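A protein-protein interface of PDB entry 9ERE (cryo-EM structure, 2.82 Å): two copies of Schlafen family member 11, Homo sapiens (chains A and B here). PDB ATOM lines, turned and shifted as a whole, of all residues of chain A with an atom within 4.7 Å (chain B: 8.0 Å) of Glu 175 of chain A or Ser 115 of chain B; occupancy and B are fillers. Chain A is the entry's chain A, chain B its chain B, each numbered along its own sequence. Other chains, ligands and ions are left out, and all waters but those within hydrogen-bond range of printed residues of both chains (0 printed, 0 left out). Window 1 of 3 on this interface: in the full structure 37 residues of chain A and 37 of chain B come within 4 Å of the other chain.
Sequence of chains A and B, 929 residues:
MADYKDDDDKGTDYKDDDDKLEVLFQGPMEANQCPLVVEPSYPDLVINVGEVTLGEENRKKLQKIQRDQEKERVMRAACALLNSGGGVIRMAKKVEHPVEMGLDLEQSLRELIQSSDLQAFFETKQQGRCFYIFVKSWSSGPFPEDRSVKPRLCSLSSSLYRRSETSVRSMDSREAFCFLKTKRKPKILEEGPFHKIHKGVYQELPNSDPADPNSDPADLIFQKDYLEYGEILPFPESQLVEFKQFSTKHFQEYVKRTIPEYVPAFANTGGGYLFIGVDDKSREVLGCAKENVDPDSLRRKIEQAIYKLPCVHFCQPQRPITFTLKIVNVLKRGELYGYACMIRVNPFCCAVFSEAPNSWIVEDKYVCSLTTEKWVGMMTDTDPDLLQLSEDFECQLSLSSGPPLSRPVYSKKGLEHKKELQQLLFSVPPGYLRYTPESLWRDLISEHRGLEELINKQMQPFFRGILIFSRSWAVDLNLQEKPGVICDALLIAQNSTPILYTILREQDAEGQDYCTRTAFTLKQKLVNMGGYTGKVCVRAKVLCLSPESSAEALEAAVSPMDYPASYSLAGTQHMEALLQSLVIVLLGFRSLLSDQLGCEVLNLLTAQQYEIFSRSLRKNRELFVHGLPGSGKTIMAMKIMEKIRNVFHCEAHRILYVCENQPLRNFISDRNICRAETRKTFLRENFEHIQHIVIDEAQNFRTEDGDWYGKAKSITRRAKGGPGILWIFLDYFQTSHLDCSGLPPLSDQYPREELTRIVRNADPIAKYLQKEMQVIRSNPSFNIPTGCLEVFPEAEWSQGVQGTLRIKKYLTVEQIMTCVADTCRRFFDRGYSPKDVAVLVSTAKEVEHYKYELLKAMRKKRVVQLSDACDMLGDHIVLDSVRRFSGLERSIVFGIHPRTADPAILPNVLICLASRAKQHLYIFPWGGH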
ATOM      1  N   ARG A 162     -11.956 -13.745 -11.355  1.00  0.00           N
ATOM      2  CA  ARG A 162     -10.746 -14.432 -11.037  1.00  0.00           C
ATOM      3  C   ARG A 162      -9.834 -13.579 -10.275  1.00  0.00           C
ATOM      4  O   ARG A 162      -9.892 -12.444 -10.435  1.00  0.00           O
ATOM      5  CB  ARG A 162     -10.028 -14.850 -12.272  1.00  0.00           C
ATOM      6  CG  ARG A 162      -9.369 -13.828 -13.133  1.00  0.00           C
ATOM      7  CD  ARG A 162      -8.564 -14.600 -14.145  1.00  0.00           C
ATOM      8  NE  ARG A 162      -9.397 -15.383 -15.030  1.00  0.00           N
ATOM      9  CZ  ARG A 162      -8.995 -16.403 -15.760  1.00  0.00           C
ATOM     10  NH1 ARG A 162      -7.746 -16.804 -15.723  1.00  0.00           N
ATOM     11  NH2 ARG A 162      -9.869 -17.014 -16.523  1.00  0.00           N
ATOM     12  N   SER A 170     -13.244  -9.288 -13.302  1.00  0.00           N
ATOM     13  CA  SER A 170     -14.358  -9.964 -13.948  1.00  0.00           C
ATOM     14  C   SER A 170     -13.957 -10.394 -15.350  1.00  0.00           C
ATOM     15  O   SER A 170     -13.461  -9.583 -16.137  1.00  0.00           O
ATOM     16  CB  SER A 170     -15.575  -9.044 -14.009  1.00  0.00           C
ATOM     17  OG  SER A 170     -16.747  -9.776 -14.315  1.00  0.00           O
ATOM     18  N   MET A 171     -14.172 -11.665 -15.666  1.00  0.00           N
ATOM     19  CA  MET A 171     -13.875 -12.151 -17.003  1.00  0.00           C
ATOM     20  C   MET A 171     -14.902 -11.625 -17.990  1.00  0.00           C
ATOM     21  O   MET A 171     -16.109 -11.743 -17.765  1.00  0.00           O
ATOM     22  CB  MET A 171     -13.864 -13.676 -17.034  1.00  0.00           C
ATOM     23  CG  MET A 171     -13.053 -14.335 -15.949  1.00  0.00           C
ATOM     24  SD  MET A 171     -13.245 -16.117 -15.986  1.00  0.00           S
ATOM     25  CE  MET A 171     -12.923 -16.512 -14.280  1.00  0.00           C
ATOM     26  N   ASP A 172     -14.425 -11.042 -19.085  1.00  0.00           N
ATOM     27  CA  ASP A 172     -15.315 -10.659 -20.166  1.00  0.00           C
ATOM     28  C   ASP A 172     -15.822 -11.917 -20.858  1.00  0.00           C
ATOM     29  O   ASP A 172     -15.572 -13.037 -20.419  1.00  0.00           O
ATOM     30  CB  ASP A 172     -14.607  -9.719 -21.139  1.00  0.00           C
ATOM     31  CG  ASP A 172     -13.238 -10.214 -21.541  1.00  0.00           C
ATOM     32  OD1 ASP A 172     -12.466 -10.598 -20.642  1.00  0.00           O
ATOM     33  OD2 ASP A 172     -12.929 -10.211 -22.750  1.00  0.00           O
ATOM     34  N   SER A 173     -16.576 -11.743 -21.940  1.00  0.00           N
ATOM     35  CA  SER A 173     -17.148 -12.906 -22.607  1.00  0.00           C
ATOM     36  C   SER A 173     -16.059 -13.828 -23.139  1.00  0.00           C
ATOM     37  O   SER A 173     -16.144 -15.047 -22.987  1.00  0.00           O
ATOM     38  CB  SER A 173     -18.083 -12.465 -23.730  1.00  0.00           C
ATOM     39  OG  SER A 173     -19.203 -11.772 -23.208  1.00  0.00           O
ATOM     40  N   ARG A 174     -15.018 -13.264 -23.747  1.00  0.00           N
ATOM     41  CA  ARG A 174     -13.940 -14.073 -24.308  1.00  0.00           C
ATOM     42  C   ARG A 174     -13.121 -14.763 -23.219  1.00  0.00           C
ATOM     43  O   ARG A 174     -12.798 -15.953 -23.334  1.00  0.00           O
ATOM     44  CB  ARG A 174     -13.057 -13.180 -25.176  1.00  0.00           C
ATOM     45  CG  ARG A 174     -11.974 -13.884 -25.947  1.00  0.00           C
ATOM     46  CD  ARG A 174     -11.131 -12.866 -26.684  1.00  0.00           C
ATOM     47  NE  ARG A 174     -11.929 -12.112 -27.646  1.00  0.00           N
ATOM     48  CZ  ARG A 174     -12.051 -10.791 -27.681  1.00  0.00           C
ATOM     49  NH1 ARG A 174     -11.437 -10.009 -26.807  1.00  0.00           N
ATOM     50  NH2 ARG A 174     -12.814 -10.236 -28.617  1.00  0.00           N
ATOM     51  N   GLU A 175     -12.790 -14.034 -22.151  1.00  0.00           N
ATOM     52  CA  GLU A 175     -12.085 -14.639 -21.027  1.00  0.00           C
ATOM     53  C   GLU A 175     -12.904 -15.757 -20.400  1.00  0.00           C
ATOM     54  O   GLU A 175     -12.366 -16.820 -20.081  1.00  0.00           O
ATOM     55  CB  GLU A 175     -11.776 -13.583 -19.973  1.00  0.00           C
ATOM     56  CG  GLU A 175     -10.542 -12.765 -20.216  1.00  0.00           C
ATOM     57  CD  GLU A 175     -10.220 -11.885 -19.031  1.00  0.00           C
ATOM     58  OE1 GLU A 175      -9.816 -12.431 -17.985  1.00  0.00           O
ATOM     59  OE2 GLU A 175     -10.389 -10.653 -19.134  1.00  0.00           O
ATOM     60  N   ALA A 176     -14.200 -15.525 -20.195  1.00  0.00           N
ATOM     61  CA  ALA A 176     -15.057 -16.537 -19.592  1.00  0.00           C
ATOM     62  C   ALA A 176     -15.224 -17.732 -20.514  1.00  0.00           C
ATOM     63  O   ALA A 176     -15.327 -18.869 -20.052  1.00  0.00           O
ATOM     64  CB  ALA A 176     -16.415 -15.933 -19.246  1.00  0.00           C
ATOM     65  N   PHE A 177     -15.259 -17.493 -21.823  1.00  0.00           N
ATOM     66  CA  PHE A 177     -15.306 -18.590 -22.778  1.00  0.00           C
ATOM     67  C   PHE A 177     -14.076 -19.472 -22.641  1.00  0.00           C
ATOM     68  O   PHE A 177     -14.184 -20.697 -22.525  1.00  0.00           O
ATOM     69  CB  PHE A 177     -15.415 -18.023 -24.190  1.00  0.00           C
ATOM     70  CG  PHE A 177     -15.448 -19.059 -25.261  1.00  0.00           C
ATOM     71  CD1 PHE A 177     -16.504 -19.940 -25.357  1.00  0.00           C
ATOM     72  CD2 PHE A 177     -14.424 -19.145 -26.182  1.00  0.00           C
ATOM     73  CE1 PHE A 177     -16.535 -20.891 -26.347  1.00  0.00           C
ATOM     74  CE2 PHE A 177     -14.451 -20.093 -27.171  1.00  0.00           C
ATOM     75  CZ  PHE A 177     -15.508 -20.966 -27.255  1.00  0.00           C
ATOM     76  N   CYS A 178     -12.892 -18.860 -22.635  1.00  0.00           N
ATOM     77  CA  CYS A 178     -11.668 -19.641 -22.481  1.00  0.00           C
ATOM     78  C   CYS A 178     -11.626 -20.345 -21.130  1.00  0.00           C
ATOM     79  O   CYS A 178     -11.183 -21.493 -21.033  1.00  0.00           O
ATOM     80  CB  CYS A 178     -10.450 -18.741 -22.659  1.00  0.00           C
ATOM     81  SG  CYS A 178     -10.287 -18.053 -24.318  1.00  0.00           S
ATOM     82  N   PHE A 179     -12.086 -19.672 -20.075  1.00  0.00           N
ATOM     83  CA  PHE A 179     -12.071 -20.257 -18.739  1.00  0.00           C
ATOM     84  C   PHE A 179     -12.985 -21.474 -18.656  1.00  0.00           C
ATOM     85  O   PHE A 179     -12.598 -22.520 -18.124  1.00  0.00           O
ATOM     86  CB  PHE A 179     -12.485 -19.191 -17.725  1.00  0.00           C
ATOM     87  CG  PHE A 179     -12.748 -19.721 -16.351  1.00  0.00           C
ATOM     88  CD1 PHE A 179     -11.710 -19.965 -15.480  1.00  0.00           C
ATOM     89  CD2 PHE A 179     -14.040 -19.955 -15.926  1.00  0.00           C
ATOM     90  CE1 PHE A 179     -11.955 -20.439 -14.216  1.00  0.00           C
ATOM     91  CE2 PHE A 179     -14.287 -20.432 -14.665  1.00  0.00           C
ATOM     92  CZ  PHE A 179     -13.245 -20.677 -13.811  1.00  0.00           C
ATOM     93  N   GLU B 106       0.522  -4.456 -12.236  1.00  0.00           N
ATOM     94  CA  GLU B 106      -0.371  -5.574 -12.519  1.00  0.00           C
ATOM     95  C   GLU B 106      -1.274  -5.263 -13.701  1.00  0.00           C
ATOM     96  O   GLU B 106      -1.469  -6.096 -14.592  1.00  0.00           O
ATOM     97  CB  GLU B 106      -1.219  -5.891 -11.290  1.00  0.00           C
ATOM     98  CG  GLU B 106      -0.469  -6.503 -10.136  1.00  0.00           C
ATOM     99  CD  GLU B 106      -1.361  -6.730  -8.934  1.00  0.00           C
ATOM    100  OE1 GLU B 106      -2.598  -6.669  -9.092  1.00  0.00           O
ATOM    101  OE2 GLU B 106      -0.826  -6.957  -7.829  1.00  0.00           O
ATOM    102  N   GLN B 107      -1.845  -4.061 -13.721  1.00  0.00           N
ATOM    103  CA  GLN B 107      -2.764  -3.709 -14.793  1.00  0.00           C
ATOM    104  C   GLN B 107      -2.035  -3.519 -16.113  1.00  0.00           C
ATOM    105  O   GLN B 107      -2.599  -3.804 -17.170  1.00  0.00           O
ATOM    106  CB  GLN B 107      -3.544  -2.448 -14.428  1.00  0.00           C
ATOM    107  CG  GLN B 107      -4.632  -2.094 -15.426  1.00  0.00           C
ATOM    108  CD  GLN B 107      -5.598  -3.237 -15.667  1.00  0.00           C
ATOM    109  OE1 GLN B 107      -5.901  -4.009 -14.760  1.00  0.00           O
ATOM    110  NE2 GLN B 107      -6.075  -3.360 -16.898  1.00  0.00           N
ATOM    111  N   SER B 108      -0.793  -3.037 -16.082  1.00  0.00           N
ATOM    112  CA  SER B 108      -0.016  -2.967 -17.312  1.00  0.00           C
ATOM    113  C   SER B 108       0.273  -4.353 -17.867  1.00  0.00           C
ATOM    114  O   SER B 108       0.189  -4.560 -19.079  1.00  0.00           O
ATOM    115  CB  SER B 108       1.282  -2.205 -17.073  1.00  0.00           C
ATOM    116  OG  SER B 108       1.019  -0.882 -16.653  1.00  0.00           O
ATOM    117  N   LEU B 109       0.603  -5.317 -17.005  1.00  0.00           N
ATOM    118  CA  LEU B 109       0.775  -6.691 -17.474  1.00  0.00           C
ATOM    119  C   LEU B 109      -0.531  -7.256 -18.022  1.00  0.00           C
ATOM    120  O   LEU B 109      -0.531  -7.986 -19.022  1.00  0.00           O
ATOM    121  CB  LEU B 109       1.300  -7.572 -16.345  1.00  0.00           C
ATOM    122  CG  LEU B 109       2.662  -7.202 -15.761  1.00  0.00           C
ATOM    123  CD1 LEU B 109       2.988  -8.105 -14.599  1.00  0.00           C
ATOM    124  CD2 LEU B 109       3.742  -7.284 -16.811  1.00  0.00           C
ATOM    125  N   ARG B 110      -1.654  -6.948 -17.368  1.00  0.00           N
ATOM    126  CA  ARG B 110      -2.950  -7.399 -17.865  1.00  0.00           C
ATOM    127  C   ARG B 110      -3.253  -6.813 -19.234  1.00  0.00           C
ATOM    128  O   ARG B 110      -3.767  -7.508 -20.109  1.00  0.00           O
ATOM    129  CB  ARG B 110      -4.058  -7.022 -16.888  1.00  0.00           C
ATOM    130  CG  ARG B 110      -4.123  -7.890 -15.664  1.00  0.00           C
ATOM    131  CD  ARG B 110      -5.292  -7.512 -14.792  1.00  0.00           C
ATOM    132  NE  ARG B 110      -5.001  -7.780 -13.392  1.00  0.00           N
ATOM    133  CZ  ARG B 110      -4.859  -6.855 -12.453  1.00  0.00           C
ATOM    134  NH1 ARG B 110      -5.008  -5.569 -12.714  1.00  0.00           N
ATOM    135  NH2 ARG B 110      -4.557  -7.232 -11.216  1.00  0.00           N
ATOM    136  N   GLU B 111      -2.971  -5.527 -19.427  1.00  0.00           N
ATOM    137  CA  GLU B 111      -3.175  -4.921 -20.736  1.00  0.00           C
ATOM    138  C   GLU B 111      -2.222  -5.511 -21.760  1.00  0.00           C
ATOM    139  O   GLU B 111      -2.557  -5.597 -22.945  1.00  0.00           O
ATOM    140  CB  GLU B 111      -2.987  -3.408 -20.654  1.00  0.00           C
ATOM    141  CG  GLU B 111      -4.165  -2.669 -20.058  1.00  0.00           C
ATOM    142  CD  GLU B 111      -3.759  -1.382 -19.372  1.00  0.00           C
ATOM    143  OE1 GLU B 111      -2.653  -0.877 -19.653  1.00  0.00           O
ATOM    144  OE2 GLU B 111      -4.546  -0.874 -18.547  1.00  0.00           O
ATOM    145  N   LEU B 112      -1.034  -5.914 -21.318  1.00  0.00           N
ATOM    146  CA  LEU B 112      -0.046  -6.506 -22.206  1.00  0.00           C
ATOM    147  C   LEU B 112      -0.523  -7.849 -22.744  1.00  0.00           C
ATOM    148  O   LEU B 112      -0.461  -8.100 -23.951  1.00  0.00           O
ATOM    149  CB  LEU B 112       1.271  -6.656 -21.448  1.00  0.00           C
ATOM    150  CG  LEU B 112       2.559  -6.943 -22.205  1.00  0.00           C
ATOM    151  CD1 LEU B 112       2.719  -5.999 -23.370  1.00  0.00           C
ATOM    152  CD2 LEU B 112       3.711  -6.805 -21.244  1.00  0.00           C
ATOM    153  N   ILE B 113      -1.020  -8.721 -21.860  1.00  0.00           N
ATOM    154  CA  ILE B 113      -1.479 -10.042 -22.286  1.00  0.00           C
ATOM    155  C   ILE B 113      -2.961 -10.073 -22.641  1.00  0.00           C
ATOM    156  O   ILE B 113      -3.474 -11.137 -23.010  1.00  0.00           O
ATOM    157  CB  ILE B 113      -1.195 -11.121 -21.220  1.00  0.00           C
ATOM    158  CG1 ILE B 113      -1.862 -10.779 -19.887  1.00  0.00           C
ATOM    159  CG2 ILE B 113       0.298 -11.296 -21.042  1.00  0.00           C
ATOM    160  CD1 ILE B 113      -2.059 -11.968 -18.988  1.00  0.00           C
ATOM    161  N   GLN B 114      -3.659  -8.942 -22.558  1.00  0.00           N
ATOM    162  CA  GLN B 114      -5.088  -8.868 -22.861  1.00  0.00           C
ATOM    163  C   GLN B 114      -5.881  -9.912 -22.086  1.00  0.00           C
ATOM    164  O   GLN B 114      -6.729 -10.613 -22.638  1.00  0.00           O
ATOM    165  CB  GLN B 114      -5.342  -9.023 -24.356  1.00  0.00           C
ATOM    166  CG  GLN B 114      -4.709  -7.967 -25.220  1.00  0.00           C
ATOM    167  CD  GLN B 114      -5.321  -7.943 -26.597  1.00  0.00           C
ATOM    168  OE1 GLN B 114      -4.643  -8.178 -27.590  1.00  0.00           O
ATOM    169  NE2 GLN B 114      -6.614  -7.661 -26.665  1.00  0.00           N
ATOM    170  N   SER B 115      -5.615 -10.015 -20.791  1.00  0.00           N
ATOM    171  CA  SER B 115      -6.278 -11.023 -19.981  1.00  0.00           C
ATOM    172  C   SER B 115      -5.963 -10.768 -18.521  1.00  0.00           C
ATOM    173  O   SER B 115      -4.868 -10.320 -18.178  1.00  0.00           O
ATOM    174  CB  SER B 115      -5.837 -12.435 -20.378  1.00  0.00           C
ATOM    175  OG  SER B 115      -6.425 -13.414 -19.542  1.00  0.00           O
ATOM    176  N   SER B 116      -6.936 -11.063 -17.665  1.00  0.00           N
ATOM    177  CA  SER B 116      -6.724 -10.988 -16.230  1.00  0.00           C
ATOM    178  C   SER B 116      -5.989 -12.204 -15.687  1.00  0.00           C
ATOM    179  O   SER B 116      -5.637 -12.215 -14.505  1.00  0.00           O
ATOM    180  CB  SER B 116      -8.066 -10.824 -15.512  1.00  0.00           C
ATOM    181  OG  SER B 116      -8.886 -11.964 -15.675  1.00  0.00           O
ATOM    182  N   ASP B 117      -5.748 -13.217 -16.521  1.00  0.00           N
ATOM    183  CA  ASP B 117      -5.008 -14.414 -16.124  1.00  0.00           C
ATOM    184  C   ASP B 117      -3.504 -14.138 -16.142  1.00  0.00           C
ATOM    185  O   ASP B 117      -2.764 -14.571 -17.023  1.00  0.00           O
ATOM    186  CB  ASP B 117      -5.365 -15.575 -17.040  1.00  0.00           C
ATOM    187  CG  ASP B 117      -5.034 -16.922 -16.434  1.00  0.00           C
ATOM    188  OD1 ASP B 117      -4.554 -16.961 -15.284  1.00  0.00           O
ATOM    189  OD2 ASP B 117      -5.256 -17.945 -17.111  1.00  0.00           O
ATOM    190  N   LEU B 118      -3.060 -13.385 -15.136  1.00  0.00           N
ATOM    191  CA  LEU B 118      -1.648 -13.035 -15.049  1.00  0.00           C
ATOM    192  C   LEU B 118      -0.791 -14.268 -14.810  1.00  0.00           C
ATOM    193  O   LEU B 118       0.284 -14.407 -15.399  1.00  0.00           O
ATOM    194  CB  LEU B 118      -1.434 -12.013 -13.934  1.00  0.00           C
ATOM    195  CG  LEU B 118      -1.792 -10.554 -14.228  1.00  0.00           C
ATOM    196  CD1 LEU B 118      -1.274  -9.666 -13.117  1.00  0.00           C
ATOM    197  CD2 LEU B 118      -1.244 -10.095 -15.557  1.00  0.00           C
ATOM    198  N   GLN B 119      -1.258 -15.183 -13.959  1.00  0.00           N
ATOM    199  CA  GLN B 119      -0.461 -16.346 -13.588  1.00  0.00           C
ATOM    200  C   GLN B 119      -0.084 -17.194 -14.790  1.00  0.00           C
ATOM    201  O   GLN B 119       0.896 -17.940 -14.726  1.00  0.00           O
ATOM    202  CB  GLN B 119      -1.231 -17.197 -12.576  1.00  0.00           C
ATOM    203  CG  GLN B 119      -0.355 -18.070 -11.692  1.00  0.00           C
ATOM    204  CD  GLN B 119       0.242 -17.311 -10.522  1.00  0.00           C
ATOM    205  OE1 GLN B 119       0.896 -16.284 -10.697  1.00  0.00           O
ATOM    206  NE2 GLN B 119       0.019 -17.818  -9.317  1.00  0.00           N
ATOM    207  N   ALA B 120      -0.839 -17.098 -15.884  1.00  0.00           N
ATOM    208  CA  ALA B 120      -0.534 -17.886 -17.070  1.00  0.00           C
ATOM    209  C   ALA B 120       0.806 -17.500 -17.677  1.00  0.00           C
ATOM    210  O   ALA B 120       1.538 -18.371 -18.154  1.00  0.00           O
ATOM    211  CB  ALA B 120      -1.640 -17.720 -18.108  1.00  0.00           C
ATOM    212  N   PHE B 121       1.138 -16.212 -17.682  1.00  0.00           N
ATOM    213  CA  PHE B 121       2.341 -15.718 -18.334  1.00  0.00           C
ATOM    214  C   PHE B 121       3.364 -15.127 -17.384  1.00  0.00           C
ATOM    215  O   PHE B 121       4.544 -15.103 -17.722  1.00  0.00           O
ATOM    216  CB  PHE B 121       1.978 -14.654 -19.374  1.00  0.00           C
ATOM    217  CG  PHE B 121       1.221 -15.196 -20.537  1.00  0.00           C
ATOM    218  CD1 PHE B 121       1.886 -15.703 -21.633  1.00  0.00           C
ATOM    219  CD2 PHE B 121      -0.159 -15.206 -20.534  1.00  0.00           C
ATOM    220  CE1 PHE B 121       1.191 -16.205 -22.700  1.00  0.00           C
ATOM    221  CE2 PHE B 121      -0.856 -15.707 -21.603  1.00  0.00           C
ATOM    222  CZ  PHE B 121      -0.181 -16.207 -22.685  1.00  0.00           C
ATOM    223  N   PHE B 122       2.951 -14.651 -16.215  1.00  0.00           N
ATOM    224  CA  PHE B 122       3.843 -13.988 -15.277  1.00  0.00           C
ATOM    225  C   PHE B 122       3.769 -14.692 -13.933  1.00  0.00           C
ATOM    226  O   PHE B 122       2.677 -14.924 -13.410  1.00  0.00           O
ATOM    227  CB  PHE B 122       3.478 -12.509 -15.124  1.00  0.00           C
ATOM    228  CG  PHE B 122       3.266 -11.805 -16.429  1.00  0.00           C
ATOM    229  CD1 PHE B 122       4.341 -11.408 -17.196  1.00  0.00           C
ATOM    230  CD2 PHE B 122       1.993 -11.553 -16.893  1.00  0.00           C
ATOM    231  CE1 PHE B 122       4.147 -10.774 -18.395  1.00  0.00           C
ATOM    232  CE2 PHE B 122       1.798 -10.920 -18.092  1.00  0.00           C
ATOM    233  CZ  PHE B 122       2.875 -10.530 -18.843  1.00  0.00           C
ATOM    234  N   TRP B 138       4.645 -15.497 -25.321  1.00  0.00           N
ATOM    235  CA  TRP B 138       3.284 -15.239 -25.770  1.00  0.00           C
ATOM    236  C   TRP B 138       2.817 -16.319 -26.734  1.00  0.00           C
ATOM    237  O   TRP B 138       1.759 -16.930 -26.538  1.00  0.00           O
ATOM    238  CB  TRP B 138       3.198 -13.863 -26.425  1.00  0.00           C
ATOM    239  CG  TRP B 138       1.851 -13.579 -26.988  1.00  0.00           C
ATOM    240  CD1 TRP B 138       1.533 -13.393 -28.294  1.00  0.00           C
ATOM    241  CD2 TRP B 138       0.630 -13.464 -26.255  1.00  0.00           C
ATOM    242  NE1 TRP B 138       0.189 -13.166 -28.426  1.00  0.00           N
ATOM    243  CE2 TRP B 138      -0.388 -13.202 -27.185  1.00  0.00           C
ATOM    244  CE3 TRP B 138       0.300 -13.554 -24.902  1.00  0.00           C
ATOM    245  CZ2 TRP B 138      -1.713 -13.030 -26.806  1.00  0.00           C
ATOM    246  CZ3 TRP B 138      -1.011 -13.386 -24.531  1.00  0.00           C
ATOM    247  CH2 TRP B 138      -2.002 -13.124 -25.476  1.00  0.00           C
ATOM    248  N   ARG B 174      -5.209  -7.929 -30.215  1.00  0.00           N
ATOM    249  CA  ARG B 174      -6.151  -8.777 -30.939  1.00  0.00           C
ATOM    250  C   ARG B 174      -6.979  -7.970 -31.933  1.00  0.00           C
ATOM    251  O   ARG B 174      -7.234  -8.426 -33.056  1.00  0.00           O
ATOM    252  CB  ARG B 174      -7.055  -9.500 -29.946  1.00  0.00           C
ATOM    253  CG  ARG B 174      -7.829 -10.650 -30.537  1.00  0.00           C
ATOM    254  CD  ARG B 174      -8.846 -11.192 -29.551  1.00  0.00           C
ATOM    255  NE  ARG B 174      -8.228 -11.640 -28.309  1.00  0.00           N
ATOM    256  CZ  ARG B 174      -8.171 -10.929 -27.190  1.00  0.00           C
ATOM    257  NH1 ARG B 174      -8.649  -9.697 -27.124  1.00  0.00           N
ATOM    258  NH2 ARG B 174      -7.620 -11.469 -26.107  1.00  0.00           N
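Printed residues of chain B within 4 Å of Arg 162 of chain A: Ser 116 and Asp 117. Printed residues of chain B within 4 Å of Arg 174 of chain A: Arg 174 (2.8 Å). Glu 175 of chain A touches just these residues of chain B: Ser 115 and Ser 116. No residue of chain B comes within 4 Å of Ala 176 of chain A. Of chain A, only Glu 175 (3.9 Å) comes within 4 Å of Ser 115 of chain B. Of the printed residues of chain A, Ser 116 of chain B touches Arg 162 (3.1 Å) and Glu 175 (2.5 Å). Of the printed residues of chain A, Asp 117 of chain B touches Arg 162. Of the printed residues of chain A, Arg 174 of chain B touches Arg 174. The nearest printed residue of chain A that does not touch Ser 115 of chain B is Arg 162 of chain A (5.3 Å).
Of the 19 printed residues of chain B, 4 touch a printed residue of chain A. Among the printed residues, Asp or Glu carboxylates within 4 Å of a Lys or Arg side-chain nitrogen of the other chain: Arg 162 of chain A with Asp 117 of chain B.
The side-chain carboxylate (OD2) of Asp 117 of chain B is in salt-bridge range of the guanidinium group (NH1) of Arg 162 of chain A (3.1 Å). OE1 of Glu 175 of chain A is in hydrogen-bond range of OG of Ser 116 of chain B, at 2.5 Å. NH1 of Arg 174 of chain B sits close to NH1 of Arg 174 of chain A (2.8 Å).
The side-chain sulfur (SD) of Met 171 of chain A lies within hydrogen-bond range of the guanidinium group (NH2) of Arg 162 of chain A, at 3.5 Å. OD1 of Asp 172 of chain A lies close to OE2 of Glu 175 of chain A, at 2.6 Å. O of Arg 174 of chain A is in hydrogen-bond range of SG of Cys 178 of chain A (3.4 Å). The backbone carbonyl oxygen of Arg 110 of chain B sits at hydrogen-bond distance from the backbone NH of Ser 115 of chain B (3.2 Å). OE1 of Gln 114 of chain B lies within hydrogen-bond range of N of Arg 174 of chain B, 2.7 Å away. OG of Ser 115 of chain B lies within hydrogen-bond range of N of Asp 117 of chain B (3.1 Å).
Arg 162 of chain A touches Ser 116 of chain B. OE1 of Glu 175 of chain A touches OG of Ser 115 of chain B, 3.9 Å away.
Arg 174 of chain A touches its own counterpart, Arg 174 of chain B.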
